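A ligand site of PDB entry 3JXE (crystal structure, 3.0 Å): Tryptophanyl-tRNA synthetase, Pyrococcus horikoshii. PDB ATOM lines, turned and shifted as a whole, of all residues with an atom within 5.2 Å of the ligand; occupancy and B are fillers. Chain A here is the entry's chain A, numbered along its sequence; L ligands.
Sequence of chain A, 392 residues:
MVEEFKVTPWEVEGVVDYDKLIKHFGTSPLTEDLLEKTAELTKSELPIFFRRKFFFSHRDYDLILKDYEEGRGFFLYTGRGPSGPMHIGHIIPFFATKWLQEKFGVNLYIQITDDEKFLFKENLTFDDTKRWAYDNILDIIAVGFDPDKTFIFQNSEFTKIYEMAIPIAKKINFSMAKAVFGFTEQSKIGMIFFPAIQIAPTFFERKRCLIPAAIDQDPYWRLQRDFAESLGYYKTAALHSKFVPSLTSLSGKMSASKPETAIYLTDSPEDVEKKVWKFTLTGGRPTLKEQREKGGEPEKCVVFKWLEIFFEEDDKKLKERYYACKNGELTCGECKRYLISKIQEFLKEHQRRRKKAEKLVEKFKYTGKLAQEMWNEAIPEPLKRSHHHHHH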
ATOM      1  N   PRO A   9      15.403 -22.714   7.776  1.00  0.00           N
ATOM      2  CA  PRO A   9      16.524 -23.654   7.815  1.00  0.00           C
ATOM      3  C   PRO A   9      16.535 -24.619   9.005  1.00  0.00           C
ATOM      4  O   PRO A   9      17.470 -25.408   9.141  1.00  0.00           O
ATOM      5  CB  PRO A   9      17.750 -22.721   7.888  1.00  0.00           C
ATOM      6  CG  PRO A   9      17.273 -21.413   7.376  1.00  0.00           C
ATOM      7  CD  PRO A   9      15.866 -21.317   7.846  1.00  0.00           C
ATOM      8  N   PHE A  54      12.098 -33.030  -9.249  1.00  0.00           N
ATOM      9  CA  PHE A  54      12.189 -32.995  -7.789  1.00  0.00           C
ATOM     10  C   PHE A  54      12.987 -31.757  -7.380  1.00  0.00           C
ATOM     11  O   PHE A  54      12.654 -31.097  -6.392  1.00  0.00           O
ATOM     12  CB  PHE A  54      12.839 -34.275  -7.249  1.00  0.00           C
ATOM     13  CG  PHE A  54      12.951 -34.315  -5.754  1.00  0.00           C
ATOM     14  CD1 PHE A  54      14.195 -34.320  -5.135  1.00  0.00           C
ATOM     15  CD2 PHE A  54      11.807 -34.338  -4.956  1.00  0.00           C
ATOM     16  CE1 PHE A  54      14.305 -34.361  -3.742  1.00  0.00           C
ATOM     17  CE2 PHE A  54      11.906 -34.379  -3.572  1.00  0.00           C
ATOM     18  CZ  PHE A  54      13.150 -34.392  -2.964  1.00  0.00           C
ATOM     19  N   TYR A  77      29.237 -26.891  -3.606  1.00  0.00           N
ATOM     20  CA  TYR A  77      29.216 -26.825  -2.153  1.00  0.00           C
ATOM     21  C   TYR A  77      27.854 -27.271  -1.629  1.00  0.00           C
ATOM     22  O   TYR A  77      26.824 -26.775  -2.055  1.00  0.00           O
ATOM     23  CB  TYR A  77      29.576 -25.421  -1.655  1.00  0.00           C
ATOM     24  CG  TYR A  77      29.062 -25.074  -0.270  1.00  0.00           C
ATOM     25  CD1 TYR A  77      29.419 -25.822   0.850  1.00  0.00           C
ATOM     26  CD2 TYR A  77      28.243 -23.966  -0.072  1.00  0.00           C
ATOM     27  CE1 TYR A  77      28.947 -25.496   2.122  1.00  0.00           C
ATOM     28  CE2 TYR A  77      27.766 -23.619   1.194  1.00  0.00           C
ATOM     29  CZ  TYR A  77      28.123 -24.391   2.279  1.00  0.00           C
ATOM     30  OH  TYR A  77      27.657 -24.050   3.532  1.00  0.00           O
ATOM     31  N   THR A  78      27.891 -28.229  -0.709  1.00  0.00           N
ATOM     32  CA  THR A  78      26.703 -28.643   0.030  1.00  0.00           C
ATOM     33  C   THR A  78      27.149 -29.027   1.443  1.00  0.00           C
ATOM     34  O   THR A  78      28.345 -29.047   1.729  1.00  0.00           O
ATOM     35  CB  THR A  78      25.935 -29.806  -0.670  1.00  0.00           C
ATOM     36  OG1 THR A  78      24.629 -29.928  -0.099  1.00  0.00           O
ATOM     37  CG2 THR A  78      26.685 -31.126  -0.554  1.00  0.00           C
ATOM     38  N   GLY A  79      26.197 -29.310   2.330  1.00  0.00           N
ATOM     39  CA  GLY A  79      26.520 -29.619   3.714  1.00  0.00           C
ATOM     40  C   GLY A  79      25.522 -30.481   4.438  1.00  0.00           C
ATOM     41  O   GLY A  79      24.504 -30.902   3.885  1.00  0.00           O
ATOM     42  N   ARG A  80      25.821 -30.742   5.712  1.00  0.00           N
ATOM     43  CA  ARG A  80      25.014 -31.611   6.558  1.00  0.00           C
ATOM     44  C   ARG A  80      25.192 -31.217   8.023  1.00  0.00           C
ATOM     45  O   ARG A  80      26.314 -31.031   8.500  1.00  0.00           O
ATOM     46  CB  ARG A  80      25.394 -33.080   6.329  1.00  0.00           C
ATOM     47  CG  ARG A  80      25.017 -34.055   7.446  1.00  0.00           C
ATOM     48  CD  ARG A  80      23.512 -34.214   7.591  1.00  0.00           C
ATOM     49  NE  ARG A  80      23.170 -34.906   8.834  1.00  0.00           N
ATOM     50  CZ  ARG A  80      21.944 -35.001   9.345  1.00  0.00           C
ATOM     51  NH1 ARG A  80      20.925 -34.431   8.723  1.00  0.00           N
ATOM     52  NH2 ARG A  80      21.754 -35.651  10.477  1.00  0.00           N
ATOM     53  N   GLY A  81      24.065 -31.093   8.730  1.00  0.00           N
ATOM     54  CA  GLY A  81      24.084 -30.839  10.167  1.00  0.00           C
ATOM     55  C   GLY A  81      23.920 -32.114  10.973  1.00  0.00           C
ATOM     56  O   GLY A  81      22.835 -32.681  11.022  1.00  0.00           O
ATOM     57  N   HIS A  87      18.750 -39.679   7.177  1.00  0.00           N
ATOM     58  CA  HIS A  87      17.681 -40.379   6.461  1.00  0.00           C
ATOM     59  C   HIS A  87      17.714 -40.119   4.948  1.00  0.00           C
ATOM     60  O   HIS A  87      18.574 -39.384   4.461  1.00  0.00           O
ATOM     61  CB  HIS A  87      16.300 -40.054   7.058  1.00  0.00           C
ATOM     62  CG  HIS A  87      15.948 -38.606   7.053  1.00  0.00           C
ATOM     63  ND1 HIS A  87      15.935 -37.838   5.912  1.00  0.00           N
ATOM     64  CD2 HIS A  87      15.561 -37.785   8.066  1.00  0.00           C
ATOM     65  CE1 HIS A  87      15.564 -36.600   6.213  1.00  0.00           C
ATOM     66  NE2 HIS A  87      15.341 -36.542   7.512  1.00  0.00           N
ATOM     67  N   GLY A  89      15.989 -38.330   2.892  1.00  0.00           N
ATOM     68  CA  GLY A  89      15.875 -36.937   2.469  1.00  0.00           C
ATOM     69  C   GLY A  89      17.199 -36.201   2.482  1.00  0.00           C
ATOM     70  O   GLY A  89      17.493 -35.429   1.570  1.00  0.00           O
ATOM     71  N   HIS A  90      18.005 -36.468   3.508  1.00  0.00           N
ATOM     72  CA  HIS A  90      19.320 -35.845   3.658  1.00  0.00           C
ATOM     73  C   HIS A  90      20.315 -36.241   2.577  1.00  0.00           C
ATOM     74  O   HIS A  90      21.220 -35.478   2.252  1.00  0.00           O
ATOM     75  CB  HIS A  90      19.924 -36.170   5.036  1.00  0.00           C
ATOM     76  CG  HIS A  90      19.111 -35.671   6.197  1.00  0.00           C
ATOM     77  ND1 HIS A  90      18.913 -36.417   7.335  1.00  0.00           N
ATOM     78  CD2 HIS A  90      18.453 -34.499   6.390  1.00  0.00           C
ATOM     79  CE1 HIS A  90      18.174 -35.727   8.188  1.00  0.00           C
ATOM     80  NE2 HIS A  90      17.872 -34.575   7.642  1.00  0.00           N
ATOM     81  N   PRO A  93      20.444 -34.503  -1.843  1.00  0.00           N
ATOM     82  CA  PRO A  93      21.350 -33.437  -2.281  1.00  0.00           C
ATOM     83  C   PRO A  93      22.738 -33.959  -2.666  1.00  0.00           C
ATOM     84  O   PRO A  93      23.308 -33.501  -3.656  1.00  0.00           O
ATOM     85  CB  PRO A  93      21.450 -32.544  -1.046  1.00  0.00           C
ATOM     86  CG  PRO A  93      20.163 -32.729  -0.356  1.00  0.00           C
ATOM     87  CD  PRO A  93      19.808 -34.172  -0.554  1.00  0.00           C
ATOM     88  N   PHE A  94      23.253 -34.917  -1.895  1.00  0.00           N
ATOM     89  CA  PHE A  94      24.578 -35.491  -2.135  1.00  0.00           C
ATOM     90  C   PHE A  94      24.648 -36.332  -3.409  1.00  0.00           C
ATOM     91  O   PHE A  94      25.687 -36.367  -4.076  1.00  0.00           O
ATOM     92  CB  PHE A  94      25.025 -36.313  -0.920  1.00  0.00           C
ATOM     93  CG  PHE A  94      25.236 -35.502   0.314  1.00  0.00           C
ATOM     94  CD1 PHE A  94      24.221 -35.374   1.260  1.00  0.00           C
ATOM     95  CD2 PHE A  94      26.440 -34.846   0.549  1.00  0.00           C
ATOM     96  CE1 PHE A  94      24.403 -34.615   2.417  1.00  0.00           C
ATOM     97  CE2 PHE A  94      26.642 -34.091   1.692  1.00  0.00           C
ATOM     98  CZ  PHE A  94      25.617 -33.972   2.628  1.00  0.00           C
ATOM     99  N   GLN A 111      30.454 -29.201   3.981  1.00  0.00           N
ATOM    100  CA  GLN A 111      30.519 -28.649   5.327  1.00  0.00           C
ATOM    101  C   GLN A 111      29.686 -29.458   6.311  1.00  0.00           C
ATOM    102  O   GLN A 111      28.485 -29.636   6.126  1.00  0.00           O
ATOM    103  CB  GLN A 111      30.081 -27.179   5.340  1.00  0.00           C
ATOM    104  CG  GLN A 111      30.309 -26.479   6.675  1.00  0.00           C
ATOM    105  CD  GLN A 111      29.625 -25.122   6.749  1.00  0.00           C
ATOM    106  OE1 GLN A 111      28.503 -24.943   6.263  1.00  0.00           O
ATOM    107  NE2 GLN A 111      30.303 -24.158   7.368  1.00  0.00           N
ATOM    108  N   THR A 113      28.347 -29.225   9.823  1.00  0.00           N
ATOM    109  CA  THR A 113      28.110 -28.168  10.791  1.00  0.00           C
ATOM    110  C   THR A 113      27.856 -28.708  12.189  1.00  0.00           C
ATOM    111  O   THR A 113      26.758 -28.567  12.740  1.00  0.00           O
ATOM    112  CB  THR A 113      26.960 -27.234  10.345  1.00  0.00           C
ATOM    113  OG1 THR A 113      25.720 -27.967  10.349  1.00  0.00           O
ATOM    114  CG2 THR A 113      27.210 -26.675   8.951  1.00  0.00           C
ATOM    115  N   GLU A 116      26.927 -25.861  14.528  1.00  0.00           N
ATOM    116  CA  GLU A 116      25.527 -25.463  14.432  1.00  0.00           C
ATOM    117  C   GLU A 116      24.649 -26.298  15.346  1.00  0.00           C
ATOM    118  O   GLU A 116      23.955 -25.756  16.208  1.00  0.00           O
ATOM    119  CB  GLU A 116      25.016 -25.595  12.993  1.00  0.00           C
ATOM    120  CG  GLU A 116      23.553 -25.192  12.815  1.00  0.00           C
ATOM    121  CD  GLU A 116      22.981 -25.603  11.462  1.00  0.00           C
ATOM    122  OE1 GLU A 116      23.695 -26.247  10.661  1.00  0.00           O
ATOM    123  OE2 GLU A 116      21.801 -25.272  11.195  1.00  0.00           O
ATOM    124  N   LYS A 117      24.723 -27.609  15.173  1.00  0.00           N
ATOM    125  CA  LYS A 117      23.816 -28.537  15.851  1.00  0.00           C
ATOM    126  C   LYS A 117      24.008 -28.606  17.359  1.00  0.00           C
ATOM    127  O   LYS A 117      23.069 -28.897  18.088  1.00  0.00           O
ATOM    128  CB  LYS A 117      23.879 -29.924  15.215  1.00  0.00           C
ATOM    129  CG  LYS A 117      23.369 -29.963  13.780  1.00  0.00           C
ATOM    130  CD  LYS A 117      22.048 -29.206  13.630  1.00  0.00           C
ATOM    131  CE  LYS A 117      21.560 -29.208  12.188  1.00  0.00           C
ATOM    132  NZ  LYS A 117      20.534 -28.150  11.969  1.00  0.00           N
ATOM    133  N   PHE A 194      26.230 -17.863  13.391  1.00  0.00           N
ATOM    134  CA  PHE A 194      26.345 -19.021  12.498  1.00  0.00           C
ATOM    135  C   PHE A 194      26.094 -18.778  10.998  1.00  0.00           C
ATOM    136  O   PHE A 194      26.819 -19.343  10.178  1.00  0.00           O
ATOM    137  CB  PHE A 194      25.515 -20.217  12.983  1.00  0.00           C
ATOM    138  CG  PHE A 194      25.566 -21.390  12.047  1.00  0.00           C
ATOM    139  CD1 PHE A 194      26.691 -22.217  11.991  1.00  0.00           C
ATOM    140  CD2 PHE A 194      24.505 -21.651  11.178  1.00  0.00           C
ATOM    141  CE1 PHE A 194      26.745 -23.284  11.102  1.00  0.00           C
ATOM    142  CE2 PHE A 194      24.559 -22.719  10.289  1.00  0.00           C
ATOM    143  CZ  PHE A 194      25.672 -23.530  10.248  1.00  0.00           C
ATOM    144  N   GLN A 198      27.962 -20.657   7.561  1.00  0.00           N
ATOM    145  CA  GLN A 198      27.369 -21.436   6.467  1.00  0.00           C
ATOM    146  C   GLN A 198      27.558 -20.771   5.101  1.00  0.00           C
ATOM    147  O   GLN A 198      27.598 -21.437   4.067  1.00  0.00           O
ATOM    148  CB  GLN A 198      25.892 -21.748   6.725  1.00  0.00           C
ATOM    149  CG  GLN A 198      25.218 -22.583   5.624  1.00  0.00           C
ATOM    150  CD  GLN A 198      24.151 -23.530   6.139  1.00  0.00           C
ATOM    151  OE1 GLN A 198      24.128 -23.886   7.315  1.00  0.00           O
ATOM    152  NE2 GLN A 198      23.268 -23.960   5.244  1.00  0.00           N
ATOM    153  N   ILE A 211      25.205 -24.590  -5.295  1.00  0.00           N
ATOM    154  CA  ILE A 211      24.765 -25.276  -4.077  1.00  0.00           C
ATOM    155  C   ILE A 211      23.514 -26.132  -4.297  1.00  0.00           C
ATOM    156  O   ILE A 211      22.389 -25.604  -4.354  1.00  0.00           O
ATOM    157  CB  ILE A 211      24.524 -24.280  -2.913  1.00  0.00           C
ATOM    158  CG1 ILE A 211      25.763 -23.409  -2.678  1.00  0.00           C
ATOM    159  CG2 ILE A 211      24.137 -25.030  -1.632  1.00  0.00           C
ATOM    160  CD1 ILE A 211      25.530 -22.224  -1.771  1.00  0.00           C
ATOM    161  N   PRO A 212      23.696 -27.458  -4.449  1.00  0.00           N
ATOM    162  CA  PRO A 212      22.570 -28.392  -4.466  1.00  0.00           C
ATOM    163  C   PRO A 212      22.070 -28.693  -3.050  1.00  0.00           C
ATOM    164  O   PRO A 212      22.789 -29.305  -2.253  1.00  0.00           O
ATOM    165  CB  PRO A 212      23.161 -29.652  -5.115  1.00  0.00           C
ATOM    166  CG  PRO A 212      24.574 -29.307  -5.501  1.00  0.00           C
ATOM    167  CD  PRO A 212      24.976 -28.166  -4.633  1.00  0.00           C
ATOM    168  N   ALA A 213      20.855 -28.256  -2.748  1.00  0.00           N
ATOM    169  CA  ALA A 213      20.219 -28.476  -1.450  1.00  0.00           C
ATOM    170  C   ALA A 213      18.699 -28.446  -1.589  1.00  0.00           C
ATOM    171  O   ALA A 213      18.174 -28.276  -2.687  1.00  0.00           O
ATOM    172  CB  ALA A 213      20.688 -27.424  -0.443  1.00  0.00           C
ATOM    173  N   ALA A 214      17.981 -28.635  -0.478  1.00  0.00           N
ATOM    174  CA  ALA A 214      16.533 -28.440  -0.487  1.00  0.00           C
ATOM    175  C   ALA A 214      16.205 -26.963  -0.245  1.00  0.00           C
ATOM    176  O   ALA A 214      17.036 -26.202   0.243  1.00  0.00           O
ATOM    177  CB  ALA A 214      15.859 -29.332   0.549  1.00  0.00           C
ATOM    178  N   ILE A 215      14.983 -26.582  -0.599  1.00  0.00           N
ATOM    179  CA  ILE A 215      14.546 -25.184  -0.537  1.00  0.00           C
ATOM    180  C   ILE A 215      14.669 -24.537   0.857  1.00  0.00           C
ATOM    181  O   ILE A 215      14.753 -23.317   0.969  1.00  0.00           O
ATOM    182  CB  ILE A 215      13.096 -25.012  -1.105  1.00  0.00           C
ATOM    183  CG1 ILE A 215      12.767 -23.544  -1.388  1.00  0.00           C
ATOM    184  CG2 ILE A 215      12.053 -25.645  -0.171  1.00  0.00           C
ATOM    185  CD1 ILE A 215      13.426 -22.977  -2.631  1.00  0.00           C
ATOM    186  N   ASP A 216      14.723 -25.361   1.900  1.00  0.00           N
ATOM    187  CA  ASP A 216      14.783 -24.858   3.280  1.00  0.00           C
ATOM    188  C   ASP A 216      16.096 -24.153   3.640  1.00  0.00           C
ATOM    189  O   ASP A 216      16.136 -23.346   4.571  1.00  0.00           O
ATOM    190  CB  ASP A 216      14.497 -25.980   4.287  1.00  0.00           C
ATOM    191  CG  ASP A 216      15.603 -27.022   4.352  1.00  0.00           C
ATOM    192  OD1 ASP A 216      16.120 -27.435   3.294  1.00  0.00           O
ATOM    193  OD2 ASP A 216      15.957 -27.429   5.478  1.00  0.00           O
ATOM    194  N   GLN A 217      17.152 -24.450   2.894  1.00  0.00           N
ATOM    195  CA  GLN A 217      18.474 -23.881   3.167  1.00  0.00           C
ATOM    196  C   GLN A 217      18.716 -22.544   2.441  1.00  0.00           C
ATOM    197  O   GLN A 217      19.777 -21.939   2.588  1.00  0.00           O
ATOM    198  CB  GLN A 217      19.581 -24.881   2.818  1.00  0.00           C
ATOM    199  CG  GLN A 217      19.593 -26.117   3.705  1.00  0.00           C
ATOM    200  CD  GLN A 217      19.795 -25.783   5.178  1.00  0.00           C
ATOM    201  OE1 GLN A 217      20.788 -25.165   5.553  1.00  0.00           O
ATOM    202  NE2 GLN A 217      18.846 -26.208   5.999  1.00  0.00           N
ATOM    203  N   TYR A 220      20.086 -18.614   3.709  1.00  0.00           N
ATOM    204  CA  TYR A 220      21.533 -18.361   3.764  1.00  0.00           C
ATOM    205  C   TYR A 220      22.048 -17.787   2.453  1.00  0.00           C
ATOM    206  O   TYR A 220      22.888 -16.874   2.452  1.00  0.00           O
ATOM    207  CB  TYR A 220      22.309 -19.641   4.068  1.00  0.00           C
ATOM    208  CG  TYR A 220      22.074 -20.241   5.422  1.00  0.00           C
ATOM    209  CD1 TYR A 220      21.219 -21.324   5.581  1.00  0.00           C
ATOM    210  CD2 TYR A 220      22.722 -19.739   6.552  1.00  0.00           C
ATOM    211  CE1 TYR A 220      21.003 -21.888   6.825  1.00  0.00           C
ATOM    212  CE2 TYR A 220      22.506 -20.295   7.808  1.00  0.00           C
ATOM    213  CZ  TYR A 220      21.647 -21.373   7.938  1.00  0.00           C
ATOM    214  OH  TYR A 220      21.429 -21.935   9.172  1.00  0.00           O
ATOM    215  N   TRP A 221      21.555 -18.325   1.342  1.00  0.00           N
ATOM    216  CA  TRP A 221      22.054 -17.962   0.029  1.00  0.00           C
ATOM    217  C   TRP A 221      21.569 -16.585  -0.419  1.00  0.00           C
ATOM    218  O   TRP A 221      22.242 -15.920  -1.205  1.00  0.00           O
ATOM    219  CB  TRP A 221      21.730 -19.041  -1.016  1.00  0.00           C
ATOM    220  CG  TRP A 221      21.831 -20.465  -0.504  1.00  0.00           C
ATOM    221  CD1 TRP A 221      20.964 -21.497  -0.765  1.00  0.00           C
ATOM    222  CD2 TRP A 221      22.855 -21.019   0.356  1.00  0.00           C
ATOM    223  NE1 TRP A 221      21.379 -22.636  -0.122  1.00  0.00           N
ATOM    224  CE2 TRP A 221      22.531 -22.372   0.569  1.00  0.00           C
ATOM    225  CE3 TRP A 221      24.001 -20.491   0.969  1.00  0.00           C
ATOM    226  CZ2 TRP A 221      23.314 -23.220   1.366  1.00  0.00           C
ATOM    227  CZ3 TRP A 221      24.780 -21.328   1.759  1.00  0.00           C
ATOM    228  CH2 TRP A 221      24.430 -22.671   1.946  1.00  0.00           C
ATOM    229  N   SER A 241      15.839 -28.511  -4.208  1.00  0.00           N
ATOM    230  CA  SER A 241      14.973 -29.682  -4.298  1.00  0.00           C
ATOM    231  C   SER A 241      13.725 -29.486  -3.446  1.00  0.00           C
ATOM    232  O   SER A 241      13.693 -28.619  -2.575  1.00  0.00           O
ATOM    233  CB  SER A 241      15.723 -30.945  -3.843  1.00  0.00           C
ATOM    234  OG  SER A 241      15.776 -31.043  -2.430  1.00  0.00           O
ATOM    235  N   LYS A 242      12.702 -30.285  -3.725  1.00  0.00           N
ATOM    236  CA  LYS A 242      11.536 -30.357  -2.860  1.00  0.00           C
ATOM    237  C   LYS A 242      11.895 -31.191  -1.621  1.00  0.00           C
ATOM    238  O   LYS A 242      13.054 -31.562  -1.430  1.00  0.00           O
ATOM    239  CB  LYS A 242      10.355 -30.981  -3.596  1.00  0.00           C
ATOM    240  CG  LYS A 242       9.736 -30.096  -4.671  1.00  0.00           C
ATOM    241  CD  LYS A 242       8.628 -30.818  -5.415  1.00  0.00           C
ATOM    242  CE  LYS A 242       8.046 -29.923  -6.504  1.00  0.00           C
ATOM    243  NZ  LYS A 242       7.011 -30.640  -7.311  1.00  0.00           N
ATOM    244  N   PHE A 243      10.893 -31.463  -0.786  1.00  0.00           N
ATOM    245  CA  PHE A 243      11.110 -32.300   0.382  1.00  0.00           C
ATOM    246  C   PHE A 243      10.614 -33.724   0.159  1.00  0.00           C
ATOM    247  O   PHE A 243       9.634 -33.945  -0.573  1.00  0.00           O
ATOM    248  CB  PHE A 243      10.421 -31.709   1.621  1.00  0.00           C
ATOM    249  CG  PHE A 243      10.932 -30.356   2.004  1.00  0.00           C
ATOM    250  CD1 PHE A 243      10.101 -29.248   1.937  1.00  0.00           C
ATOM    251  CD2 PHE A 243      12.248 -30.184   2.437  1.00  0.00           C
ATOM    252  CE1 PHE A 243      10.566 -27.982   2.292  1.00  0.00           C
ATOM    253  CE2 PHE A 243      12.717 -28.929   2.800  1.00  0.00           C
ATOM    254  CZ  PHE A 243      11.874 -27.822   2.724  1.00  0.00           C
ATOM    255  N   VAL A 244      11.294 -34.679   0.769  1.00  0.00           N
ATOM    256  CA  VAL A 244      10.803 -36.050   0.852  1.00  0.00           C
ATOM    257  C   VAL A 244       9.790 -36.095   1.995  1.00  0.00           C
ATOM    258  O   VAL A 244      10.141 -35.788   3.130  1.00  0.00           O
ATOM    259  CB  VAL A 244      11.946 -37.060   1.102  1.00  0.00           C
ATOM    260  CG1 VAL A 244      11.399 -38.481   1.226  1.00  0.00           C
ATOM    261  CG2 VAL A 244      12.970 -36.998  -0.009  1.00  0.00           C
ATOM    262  N   LYS A 253       7.451 -32.791   6.509  1.00  0.00           N
ATOM    263  CA  LYS A 253       8.775 -33.100   5.986  1.00  0.00           C
ATOM    264  C   LYS A 253       9.303 -34.312   6.742  1.00  0.00           C
ATOM    265  O   LYS A 253       9.058 -34.438   7.952  1.00  0.00           O
ATOM    266  CB  LYS A 253       9.699 -31.890   6.196  1.00  0.00           C
ATOM    267  CG  LYS A 253      11.205 -32.127   6.107  1.00  0.00           C
ATOM    268  CD  LYS A 253      11.928 -31.179   7.055  1.00  0.00           C
ATOM    269  CE  LYS A 253      13.395 -31.008   6.713  1.00  0.00           C
ATOM    270  NZ  LYS A 253      14.200 -32.185   7.101  1.00  0.00           N
ATOM    271  N   MET A 254       9.995 -35.212   6.056  1.00  0.00           N
ATOM    272  CA  MET A 254      10.600 -36.359   6.718  1.00  0.00           C
ATOM    273  C   MET A 254      11.695 -35.886   7.659  1.00  0.00           C
ATOM    274  O   MET A 254      12.704 -35.321   7.232  1.00  0.00           O
ATOM    275  CB  MET A 254      11.145 -37.379   5.717  1.00  0.00           C
ATOM    276  CG  MET A 254      11.665 -38.656   6.371  1.00  0.00           C
ATOM    277  SD  MET A 254      11.940 -40.024   5.232  1.00  0.00           S
ATOM    278  CE  MET A 254      13.486 -39.549   4.487  1.00  0.00           C
HETATM  279  P1  LIG L   1      20.402 -30.655   7.261  1.00  0.00           P
HETATM  280  O1  LIG L   1      21.424 -31.509   7.906  1.00  0.00           O
HETATM  281  O2  LIG L   1      19.167 -30.308   7.993  1.00  0.00           O
HETATM  282  O3  LIG L   1      19.933 -31.362   5.882  1.00  0.00           O
HETATM  283  C1  LIG L   1      20.918 -31.890   4.975  1.00  0.00           C
HETATM  284  C2  LIG L   1      20.513 -31.683   3.504  1.00  0.00           C
HETATM  285  O4  LIG L   1      19.305 -32.409   3.196  1.00  0.00           O
HETATM  286  C3  LIG L   1      18.277 -31.478   2.730  1.00  0.00           C
HETATM  287  N1  LIG L   1      17.042 -32.039   3.328  1.00  0.00           N
HETATM  288  C4  LIG L   1      16.068 -32.669   2.670  1.00  0.00           C
HETATM  289  N2  LIG L   1      15.851 -32.971   1.380  1.00  0.00           N
HETATM  290  C5  LIG L   1      14.763 -33.628   1.003  1.00  0.00           C
HETATM  291  N3  LIG L   1      13.830 -34.000   1.882  1.00  0.00           N
HETATM  292  C6  LIG L   1      13.983 -33.724   3.188  1.00  0.00           C
HETATM  293  N4  LIG L   1      13.048 -34.094   4.057  1.00  0.00           N
HETATM  294  C7  LIG L   1      15.111 -33.038   3.615  1.00  0.00           C
HETATM  295  N5  LIG L   1      15.549 -32.629   4.794  1.00  0.00           N
HETATM  296  C8  LIG L   1      16.724 -32.020   4.625  1.00  0.00           C
HETATM  297  C9  LIG L   1      18.717 -30.103   3.242  1.00  0.00           C
HETATM  298  O5  LIG L   1      18.267 -29.078   2.359  1.00  0.00           O
HETATM  299  C10 LIG L   1      20.238 -30.205   3.173  1.00  0.00           C
HETATM  300  O6  LIG L   1      20.705 -29.940   1.849  1.00  0.00           O
HETATM  301  N6  LIG L   1      22.488 -26.291   8.261  1.00  0.00           N
HETATM  302  C11 LIG L   1      22.513 -27.374   7.272  1.00  0.00           C
HETATM  303  C12 LIG L   1      23.955 -27.842   7.082  1.00  0.00           C
HETATM  304  C13 LIG L   1      24.631 -27.152   5.867  1.00  0.00           C
HETATM  305  C14 LIG L   1      24.226 -27.140   4.538  1.00  0.00           C
HETATM  306  C15 LIG L   1      25.154 -26.385   3.807  1.00  0.00           C
HETATM  307  C16 LIG L   1      23.139 -27.721   3.886  1.00  0.00           C
HETATM  308  C17 LIG L   1      25.772 -26.415   5.900  1.00  0.00           C
HETATM  309  N7  LIG L   1      26.094 -25.929   4.626  1.00  0.00           N
HETATM  310  C18 LIG L   1      24.987 -26.213   2.436  1.00  0.00           C
HETATM  311  C19 LIG L   1      22.970 -27.549   2.504  1.00  0.00           C
HETATM  312  C20 LIG L   1      23.900 -26.794   1.784  1.00  0.00           C
HETATM  313  C21 LIG L   1      21.658 -28.554   7.754  1.00  0.00           C
HETATM  314  O7  LIG L   1      21.513 -28.762   8.954  1.00  0.00           O
HETATM  315  O8  LIG L   1      21.109 -29.299   6.740  1.00  0.00           O
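N2 of the ligand sits close to O of Gly 89 (3.0 Å).
Merely in contact with the ligand: Gly 79 (3.3 Å), Thr 113 (3.4 Å), Ala 213 (3.4 Å), His 90 (3.5 Å), Phe 243 (3.5 Å), Trp 221 (3.6 Å), Pro 93 (3.6 Å), Lys 242 (3.6 Å), Thr 78 (3.7 Å) and Ile 211 (3.9 Å).
Hydrophobic or aromatic side chains that line the ligand: Tyr 77, His 90, Pro 93, Ile 211, Ala 213, Ala 214, Trp 221 and Val 244.
A ring nitrogen (NE2) of His 90 sits close to a ring nitrogen (NE2) of His 87 (3.2 Å).
The side-chain hydroxyl (OG1) of Thr 78 sits at hydrogen-bond distance from the backbone carbonyl oxygen (O) of Pro 212, 2.9 Å away.
The backbone NH (N) of Arg 80 sits at hydrogen-bond distance from the backbone carbonyl oxygen (O) of Gln 111.
The side-chain carboxylate of Asp 216 is in hydrogen-bond range of the side-chain amide nitrogen of Gln 217, at 3.2 Å.
O of Val 244 is in hydrogen-bond range of N of Met 254 (3.0 Å).
The side-chain carboxylate (OE2) of Glu 116 lies within salt-bridge range of the side-chain amino group (NZ) of Lys 117, 3.2 Å away.
The backbone carbonyl oxygen (O) of Arg 80 is in hydrogen-bond range of the backbone NH (N) of Thr 113 (3.0 Å).
The backbone NH of Ser 241 is in hydrogen-bond range of the backbone carbonyl oxygen of Ala 213.
OH of Tyr 77 sits at hydrogen-bond distance from N7 of the ligand, at 2.7 Å.
N of Val 244 lies within hydrogen-bond range of N3 of the ligand (2.9 Å).
The side-chain carboxylate (OE1) of Glu 116 lies within salt-bridge range of a nitrogen (N6) of the ligand (2.7 Å).
The backbone NH (N) of Gly 81 sits at hydrogen-bond distance from an oxygen (O1) of the ligand, at 2.8 Å.
OD1 of Asp 216 sits at hydrogen-bond distance from O5 of the ligand (2.9 Å).
O of Val 244 lies within hydrogen-bond range of N4 of the ligand.
The side-chain amino group of Lys 253 is in hydrogen-bond range of a nitrogen (N5) of the ligand (2.7 Å).
The side-chain amide oxygen of Gln 217 sits close to a nitrogen (N6) of the ligand (3.4 Å).
The side-chain amide oxygen (OE1) of Gln 198 is in hydrogen-bond range of a nitrogen (N6) of the ligand, at 3.1 Å.
A nitrogen (N4) of the ligand is in hydrogen-bond range of the backbone carbonyl oxygen (O) of Met 254 (3.4 Å).
A nitrogen (N7) of the ligand sits at hydrogen-bond distance from the side-chain amide oxygen of Gln 111, 3.1 Å away.
NZ of Lys 117 lies within hydrogen-bond range of O7 of the ligand, at 3.2 Å.
An oxygen (O5) of the ligand lies within hydrogen-bond range of the backbone NH (N) of Ala 214 (2.9 Å).
The guanidinium group of Arg 80 lies within salt-bridge range of an oxygen (O1) of the ligand, 3.1 Å away.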
